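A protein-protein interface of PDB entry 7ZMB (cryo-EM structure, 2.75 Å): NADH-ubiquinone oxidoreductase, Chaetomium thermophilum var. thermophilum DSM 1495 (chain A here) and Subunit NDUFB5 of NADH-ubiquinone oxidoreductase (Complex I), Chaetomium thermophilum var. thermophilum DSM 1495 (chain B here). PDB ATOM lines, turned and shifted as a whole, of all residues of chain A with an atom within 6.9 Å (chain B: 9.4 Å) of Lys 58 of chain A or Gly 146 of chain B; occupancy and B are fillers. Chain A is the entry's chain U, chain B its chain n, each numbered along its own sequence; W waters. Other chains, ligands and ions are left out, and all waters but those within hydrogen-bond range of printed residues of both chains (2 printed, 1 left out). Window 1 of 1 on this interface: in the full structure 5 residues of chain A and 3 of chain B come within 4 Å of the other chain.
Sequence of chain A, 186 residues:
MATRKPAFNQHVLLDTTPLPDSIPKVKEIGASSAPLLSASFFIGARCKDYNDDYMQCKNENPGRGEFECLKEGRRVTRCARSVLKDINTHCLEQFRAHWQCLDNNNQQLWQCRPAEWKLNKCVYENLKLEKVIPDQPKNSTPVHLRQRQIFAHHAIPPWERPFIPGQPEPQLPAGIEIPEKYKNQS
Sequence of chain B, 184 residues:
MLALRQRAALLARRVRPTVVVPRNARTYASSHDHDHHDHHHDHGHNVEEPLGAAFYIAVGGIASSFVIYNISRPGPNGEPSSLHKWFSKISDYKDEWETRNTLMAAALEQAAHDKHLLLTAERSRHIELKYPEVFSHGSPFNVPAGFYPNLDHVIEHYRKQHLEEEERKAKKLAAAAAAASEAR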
ATOM      1  N   ASP A  53       6.684 -19.504  23.279  1.00  0.00           N
ATOM      2  CA  ASP A  53       6.453 -18.613  22.114  1.00  0.00           C
ATOM      3  C   ASP A  53       6.289 -19.483  20.871  1.00  0.00           C
ATOM      4  O   ASP A  53       5.405 -19.175  20.058  1.00  0.00           O
ATOM      5  CB  ASP A  53       7.598 -17.625  21.922  1.00  0.00           C
ATOM      6  CG  ASP A  53       7.235 -16.420  21.076  1.00  0.00           C
ATOM      7  OD1 ASP A  53       6.083 -15.965  21.174  1.00  0.00           O
ATOM      8  OD2 ASP A  53       8.112 -15.948  20.327  1.00  0.00           O
ATOM      9  N   TYR A  54       7.135 -20.505  20.731  1.00  0.00           N
ATOM     10  CA  TYR A  54       7.014 -21.473  19.607  1.00  0.00           C
ATOM     11  C   TYR A  54       5.595 -22.040  19.551  1.00  0.00           C
ATOM     12  O   TYR A  54       4.960 -21.947  18.500  1.00  0.00           O
ATOM     13  CB  TYR A  54       8.139 -22.508  19.672  1.00  0.00           C
ATOM     14  CG  TYR A  54       8.178 -23.475  18.520  1.00  0.00           C
ATOM     15  CD1 TYR A  54       8.286 -23.017  17.221  1.00  0.00           C
ATOM     16  CD2 TYR A  54       8.107 -24.841  18.726  1.00  0.00           C
ATOM     17  CE1 TYR A  54       8.323 -23.889  16.151  1.00  0.00           C
ATOM     18  CE2 TYR A  54       8.144 -25.730  17.665  1.00  0.00           C
ATOM     19  CZ  TYR A  54       8.253 -25.248  16.374  1.00  0.00           C
ATOM     20  OH  TYR A  54       8.287 -26.094  15.308  1.00  0.00           O
ATOM     21  N   MET A  55       5.143 -22.655  20.637  1.00  0.00           N
ATOM     22  CA  MET A  55       3.822 -23.327  20.707  1.00  0.00           C
ATOM     23  C   MET A  55       2.650 -22.359  20.472  1.00  0.00           C
ATOM     24  O   MET A  55       1.671 -22.803  19.870  1.00  0.00           O
ATOM     25  CB  MET A  55       3.695 -24.045  22.054  1.00  0.00           C
ATOM     26  CG  MET A  55       4.854 -24.963  22.360  1.00  0.00           C
ATOM     27  SD  MET A  55       4.868 -26.420  21.304  1.00  0.00           S
ATOM     28  CE  MET A  55       3.438 -27.293  21.937  1.00  0.00           C
ATOM     29  N   GLN A  56       2.750 -21.103  20.923  1.00  0.00           N
ATOM     30  CA  GLN A  56       1.682 -20.086  20.747  1.00  0.00           C
ATOM     31  C   GLN A  56       1.689 -19.639  19.287  1.00  0.00           C
ATOM     32  O   GLN A  56       0.597 -19.383  18.755  1.00  0.00           O
ATOM     33  CB  GLN A  56       1.882 -18.887  21.661  1.00  0.00           C
ATOM     34  CG  GLN A  56       1.287 -19.068  23.047  1.00  0.00           C
ATOM     35  CD  GLN A  56       1.683 -17.941  23.966  1.00  0.00           C
ATOM     36  OE1 GLN A  56       2.675 -17.254  23.744  1.00  0.00           O
ATOM     37  NE2 GLN A  56       0.903 -17.744  25.014  1.00  0.00           N
ATOM     38  N   CYS A  57       2.855 -19.621  18.652  1.00  0.00           N
ATOM     39  CA  CYS A  57       2.925 -19.318  17.205  1.00  0.00           C
ATOM     40  C   CYS A  57       2.222 -20.428  16.416  1.00  0.00           C
ATOM     41  O   CYS A  57       1.460 -20.101  15.503  1.00  0.00           O
ATOM     42  CB  CYS A  57       4.383 -19.203  16.772  1.00  0.00           C
ATOM     43  SG  CYS A  57       4.607 -18.769  15.028  1.00  0.00           S
ATOM     44  N   LYS A  58       2.484 -21.695  16.746  1.00  0.00           N
ATOM     45  CA  LYS A  58       1.865 -22.832  16.018  1.00  0.00           C
ATOM     46  C   LYS A  58       0.345 -22.795  16.206  1.00  0.00           C
ATOM     47  O   LYS A  58      -0.361 -23.040  15.226  1.00  0.00           O
ATOM     48  CB  LYS A  58       2.562 -24.145  16.379  1.00  0.00           C
ATOM     49  CG  LYS A  58       4.033 -24.212  15.997  1.00  0.00           C
ATOM     50  CD  LYS A  58       4.618 -25.592  16.144  1.00  0.00           C
ATOM     51  CE  LYS A  58       3.995 -26.600  15.204  1.00  0.00           C
ATOM     52  NZ  LYS A  58       4.611 -27.936  15.367  1.00  0.00           N
ATOM     53  N   ASN A  59      -0.124 -22.455  17.405  1.00  0.00           N
ATOM     54  CA  ASN A  59      -1.579 -22.352  17.698  1.00  0.00           C
ATOM     55  C   ASN A  59      -2.117 -21.067  17.057  1.00  0.00           C
ATOM     56  O   ASN A  59      -3.341 -20.948  16.962  1.00  0.00           O
ATOM     57  CB  ASN A  59      -1.854 -22.407  19.199  1.00  0.00           C
ATOM     58  CG  ASN A  59      -1.957 -23.805  19.760  1.00  0.00           C
ATOM     59  OD1 ASN A  59      -1.336 -24.727  19.248  1.00  0.00           O
ATOM     60  ND2 ASN A  59      -2.731 -23.970  20.818  1.00  0.00           N
ATOM     61  N   GLU A  60      -1.240 -20.173  16.584  1.00  0.00           N
ATOM     62  CA  GLU A  60      -1.696 -18.993  15.868  1.00  0.00           C
ATOM     63  C   GLU A  60      -1.795 -19.215  14.369  1.00  0.00           C
ATOM     64  O   GLU A  60      -2.435 -18.416  13.682  1.00  0.00           O
ATOM     65  CB  GLU A  60      -0.757 -17.826  16.147  1.00  0.00           C
ATOM     66  CG  GLU A  60      -1.389 -16.462  16.049  1.00  0.00           C
ATOM     67  CD  GLU A  60      -0.420 -15.361  16.422  1.00  0.00           C
ATOM     68  OE1 GLU A  60      -0.224 -14.435  15.606  1.00  0.00           O
ATOM     69  OE2 GLU A  60       0.152 -15.427  17.529  1.00  0.00           O
ATOM     70  N   ASN A  61      -1.185 -20.275  13.846  1.00  0.00           N
ATOM     71  CA  ASN A  61      -1.274 -20.636  12.431  1.00  0.00           C
ATOM     72  C   ASN A  61      -1.634 -22.110  12.321  1.00  0.00           C
ATOM     73  O   ASN A  61      -0.764 -22.957  12.075  1.00  0.00           O
ATOM     74  CB  ASN A  61       0.035 -20.344  11.697  1.00  0.00           C
ATOM     75  CG  ASN A  61       0.591 -18.983  12.018  1.00  0.00           C
ATOM     76  OD1 ASN A  61       1.469 -18.842  12.864  1.00  0.00           O
ATOM     77  ND2 ASN A  61       0.087 -17.966  11.335  1.00  0.00           N
ATOM     78  N   PRO A  62      -2.907 -22.454  12.497  1.00  0.00           N
ATOM     79  CA  PRO A  62      -3.297 -23.871  12.458  1.00  0.00           C
ATOM     80  C   PRO A  62      -3.117 -24.470  11.070  1.00  0.00           C
ATOM     81  O   PRO A  62      -3.574 -23.916  10.071  1.00  0.00           O
ATOM     82  CB  PRO A  62      -4.771 -23.842  12.878  1.00  0.00           C
ATOM     83  CG  PRO A  62      -4.909 -22.569  13.648  1.00  0.00           C
ATOM     84  CD  PRO A  62      -4.007 -21.599  12.958  1.00  0.00           C
ATOM     85  N   GLY A  63      -2.442 -25.616  11.022  1.00  0.00           N
ATOM     86  CA  GLY A  63      -2.143 -26.293   9.784  1.00  0.00           C
ATOM     87  C   GLY A  63      -0.925 -25.783   9.058  1.00  0.00           C
ATOM     88  O   GLY A  63      -0.549 -26.363   8.037  1.00  0.00           O
ATOM     89  N   ARG A  64      -0.297 -24.718   9.547  1.00  0.00           N
ATOM     90  CA  ARG A  64       0.813 -24.060   8.871  1.00  0.00           C
ATOM     91  C   ARG A  64       1.963 -23.794   9.829  1.00  0.00           C
ATOM     92  O   ARG A  64       2.856 -23.005   9.513  1.00  0.00           O
ATOM     93  CB  ARG A  64       0.356 -22.742   8.243  1.00  0.00           C
ATOM     94  CG  ARG A  64      -0.720 -22.866   7.198  1.00  0.00           C
ATOM     95  CD  ARG A  64      -0.124 -23.239   5.885  1.00  0.00           C
ATOM     96  NE  ARG A  64       1.199 -22.654   5.714  1.00  0.00           N
ATOM     97  CZ  ARG A  64       2.034 -22.979   4.736  1.00  0.00           C
ATOM     98  NH1 ARG A  64       1.680 -23.887   3.841  1.00  0.00           N
ATOM     99  NH2 ARG A  64       3.219 -22.400   4.651  1.00  0.00           N
ATOM    100  N   GLY A  65       1.893 -24.347  11.039  1.00  0.00           N
ATOM    101  CA  GLY A  65       2.917 -24.029  12.050  1.00  0.00           C
ATOM    102  C   GLY A  65       4.295 -24.448  11.598  1.00  0.00           C
ATOM    103  O   GLY A  65       5.252 -23.706  11.866  1.00  0.00           O
ATOM    104  N   GLU A  66       4.394 -25.576  10.896  1.00  0.00           N
ATOM    105  CA  GLU A  66       5.731 -26.096  10.529  1.00  0.00           C
ATOM    106  C   GLU A  66       6.447 -25.062   9.663  1.00  0.00           C
ATOM    107  O   GLU A  66       7.625 -24.786   9.950  1.00  0.00           O
ATOM    108  CB  GLU A  66       5.598 -27.416   9.765  1.00  0.00           C
ATOM    109  CG  GLU A  66       5.112 -28.582  10.603  1.00  0.00           C
ATOM    110  CD  GLU A  66       3.610 -28.810  10.596  1.00  0.00           C
ATOM    111  OE1 GLU A  66       2.870 -27.928  10.112  1.00  0.00           O
ATOM    112  OE2 GLU A  66       3.185 -29.879  11.068  1.00  0.00           O
ATOM    113  N   CYS A  69       6.491 -20.885  11.601  1.00  0.00           N
ATOM    114  CA  CYS A  69       7.077 -20.556  12.927  1.00  0.00           C
ATOM    115  C   CYS A  69       8.540 -21.008  13.003  1.00  0.00           C
ATOM    116  O   CYS A  69       8.989 -21.372  14.099  1.00  0.00           O
ATOM    117  CB  CYS A  69       6.238 -21.161  14.044  1.00  0.00           C
ATOM    118  SG  CYS A  69       4.533 -20.554  14.049  1.00  0.00           S
ATOM    119  N   VAL B 143      -2.535 -33.114  22.356  1.00  0.00           N
ATOM    120  CA  VAL B 143      -2.942 -32.247  21.224  1.00  0.00           C
ATOM    121  C   VAL B 143      -1.671 -31.699  20.593  1.00  0.00           C
ATOM    122  O   VAL B 143      -0.873 -31.093  21.308  1.00  0.00           O
ATOM    123  CB  VAL B 143      -3.929 -31.152  21.672  1.00  0.00           C
ATOM    124  CG1 VAL B 143      -4.274 -30.188  20.552  1.00  0.00           C
ATOM    125  CG2 VAL B 143      -5.183 -31.748  22.285  1.00  0.00           C
ATOM    126  N   PRO B 144      -1.452 -31.909  19.281  1.00  0.00           N
ATOM    127  CA  PRO B 144      -0.303 -31.305  18.611  1.00  0.00           C
ATOM    128  C   PRO B 144      -0.552 -29.792  18.623  1.00  0.00           C
ATOM    129  O   PRO B 144      -1.691 -29.409  18.594  1.00  0.00           O
ATOM    130  CB  PRO B 144      -0.367 -31.923  17.207  1.00  0.00           C
ATOM    131  CG  PRO B 144      -1.267 -33.123  17.341  1.00  0.00           C
ATOM    132  CD  PRO B 144      -2.269 -32.737  18.401  1.00  0.00           C
ATOM    133  N   ALA B 145       0.488 -28.969  18.708  1.00  0.00           N
ATOM    134  CA  ALA B 145       0.266 -27.504  18.606  1.00  0.00           C
ATOM    135  C   ALA B 145      -0.221 -27.137  17.206  1.00  0.00           C
ATOM    136  O   ALA B 145       0.353 -27.637  16.224  1.00  0.00           O
ATOM    137  CB  ALA B 145       1.501 -26.736  18.962  1.00  0.00           C
ATOM    138  N   GLY B 146      -1.236 -26.278  17.128  1.00  0.00           N
ATOM    139  CA  GLY B 146      -1.794 -25.849  15.839  1.00  0.00           C
ATOM    140  C   GLY B 146      -2.621 -26.913  15.163  1.00  0.00           C
ATOM    141  O   GLY B 146      -2.891 -26.771  13.967  1.00  0.00           O
ATOM    142  N   PHE B 147      -3.023 -27.939  15.900  1.00  0.00           N
ATOM    143  CA  PHE B 147      -3.889 -28.984  15.305  1.00  0.00           C
ATOM    144  C   PHE B 147      -5.320 -28.465  15.117  1.00  0.00           C
ATOM    145  O   PHE B 147      -5.857 -28.566  14.007  1.00  0.00           O
ATOM    146  CB  PHE B 147      -3.827 -30.250  16.157  1.00  0.00           C
ATOM    147  CG  PHE B 147      -4.857 -31.294  15.823  1.00  0.00           C
ATOM    148  CD1 PHE B 147      -6.134 -31.224  16.357  1.00  0.00           C
ATOM    149  CD2 PHE B 147      -4.541 -32.356  14.995  1.00  0.00           C
ATOM    150  CE1 PHE B 147      -7.087 -32.171  16.038  1.00  0.00           C
ATOM    151  CE2 PHE B 147      -5.490 -33.319  14.697  1.00  0.00           C
ATOM    152  CZ  PHE B 147      -6.755 -33.223  15.223  1.00  0.00           C
ATOM    153  N   TYR B 148      -5.878 -27.841  16.146  1.00  0.00           N
ATOM    154  CA  TYR B 148      -7.301 -27.421  16.088  1.00  0.00           C
ATOM    155  C   TYR B 148      -7.462 -26.151  15.245  1.00  0.00           C
ATOM    156  O   TYR B 148      -6.619 -25.250  15.367  1.00  0.00           O
ATOM    157  CB  TYR B 148      -7.889 -27.203  17.482  1.00  0.00           C
ATOM    158  CG  TYR B 148      -8.216 -28.461  18.243  1.00  0.00           C
ATOM    159  CD1 TYR B 148      -9.217 -29.314  17.816  1.00  0.00           C
ATOM    160  CD2 TYR B 148      -7.535 -28.789  19.400  1.00  0.00           C
ATOM    161  CE1 TYR B 148      -9.522 -30.471  18.512  1.00  0.00           C
ATOM    162  CE2 TYR B 148      -7.829 -29.939  20.110  1.00  0.00           C
ATOM    163  CZ  TYR B 148      -8.823 -30.786  19.661  1.00  0.00           C
ATOM    164  OH  TYR B 148      -9.111 -31.924  20.350  1.00  0.00           O
ATOM    165  N   PRO B 149      -8.483 -26.027  14.365  1.00  0.00           N
ATOM    166  CA  PRO B 149      -8.696 -24.766  13.656  1.00  0.00           C
ATOM    167  C   PRO B 149      -9.309 -23.720  14.569  1.00  0.00           C
ATOM    168  O   PRO B 149      -9.935 -24.021  15.585  1.00  0.00           O
ATOM    169  CB  PRO B 149      -9.659 -25.147  12.530  1.00  0.00           C
ATOM    170  CG  PRO B 149     -10.377 -26.300  13.045  1.00  0.00           C
ATOM    171  CD  PRO B 149      -9.444 -27.056  13.941  1.00  0.00           C
ATOM    172  N   ASN B 150      -9.108 -22.466  14.190  1.00  0.00           N
ATOM    173  CA  ASN B 150      -9.634 -21.350  14.958  1.00  0.00           C
ATOM    174  C   ASN B 150     -11.075 -21.121  14.529  1.00  0.00           C
ATOM    175  O   ASN B 150     -11.329 -20.602  13.438  1.00  0.00           O
ATOM    176  CB  ASN B 150      -8.771 -20.112  14.738  1.00  0.00           C
ATOM    177  CG  ASN B 150      -9.170 -18.953  15.618  1.00  0.00           C
ATOM    178  OD1 ASN B 150     -10.346 -18.626  15.745  1.00  0.00           O
ATOM    179  ND2 ASN B 150      -8.183 -18.319  16.238  1.00  0.00           N
HETATM  180  O   HOH W   1       2.930 -29.432  17.117  1.00  0.00           O
HETATM  181  O   HOH W   2      -1.145 -28.267  12.374  1.00  0.00           O
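OD1 of Asn 59 of chain A is in hydrogen-bond range of N of Gly 146 of chain B. The backbone carbonyl oxygen (O) of Gly 146 of chain B sits at hydrogen-bond distance from the backbone NH (N) of Gly 63 of chain A (3.2 Å).
The side-chain sulfur of Cys 57 of chain A forms a disulfide with the side-chain sulfur of Cys 69 of chain A. The side-chain sulfur of Cys 69 of chain A is in hydrogen-bond range of the backbone NH of Lys 58 of chain A, at 3.6 Å.
Among the printed residues, merely in contact across the chains: Met 55 of chain A with Ala 145 of chain B, Lys 58 of chain A with Ala 145 of chain B, Lys 58 of chain A with Gly 146 of chain B, Asn 59 of chain A with Ala 145 of chain B, Pro 62 of chain A with Gly 146 of chain B and Pro 62 of chain A with Tyr 148 of chain B.
Lys 58 of chain A touches just these residues of chain B: Ala 145 (3.8 Å) and Gly 146 (3.2 Å). Gly 146 of chain B touches just these residues of chain A: Lys 58, Asn 59, Pro 62 and Gly 63. Asn 59 of chain A touches just these residues of chain B: Ala 145 and Gly 146. Of chain B, only Gly 146 (3.3 Å) and Tyr 148 (3.4 Å) come within 4 Å of Pro 62 of chain A. No residue of chain B comes within 4 Å of Gly 65 of chain A. Printed residues of chain A within 4 Å of Ala 145 of chain B: Met 55, Lys 58 and Asn 59. Of the printed residues of chain A, Tyr 148 of chain B touches Pro 62. Printed residues of chain B within 4 Å of Met 55 of chain A: Ala 145. Of the printed residues of chain B, Gly 63 of chain A touches Gly 146. Gln 56 of chain A touches none of the printed residues of chain B. Val 143 of chain B touches none of the printed residues of chain A. The nearest residue of chain A that does not touch Gly 146 of chain B is Asn 61 of chain A (4.8 Å).
Of the 15 printed residues of chain A, 5 touch a printed residue of chain B. Hydrophobic or aromatic side chains of chain B that line the printed part of chain A: Ala 145. Along chain B the printed residues that touch a printed residue of chain A span positions 145 to 148. Among the printed residues, 8 pairs touch across the chains.
Water W2 bridges the backbone carbonyl oxygen (O) of Gly 146 of chain B (2.8 Å) and the backbone NH (N) of Gly 63 of chain A (3.2 Å). Water W1 lies within hydrogen-bond range of NZ of Lys 58 of chain A and N of Ala 145 of chain B.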
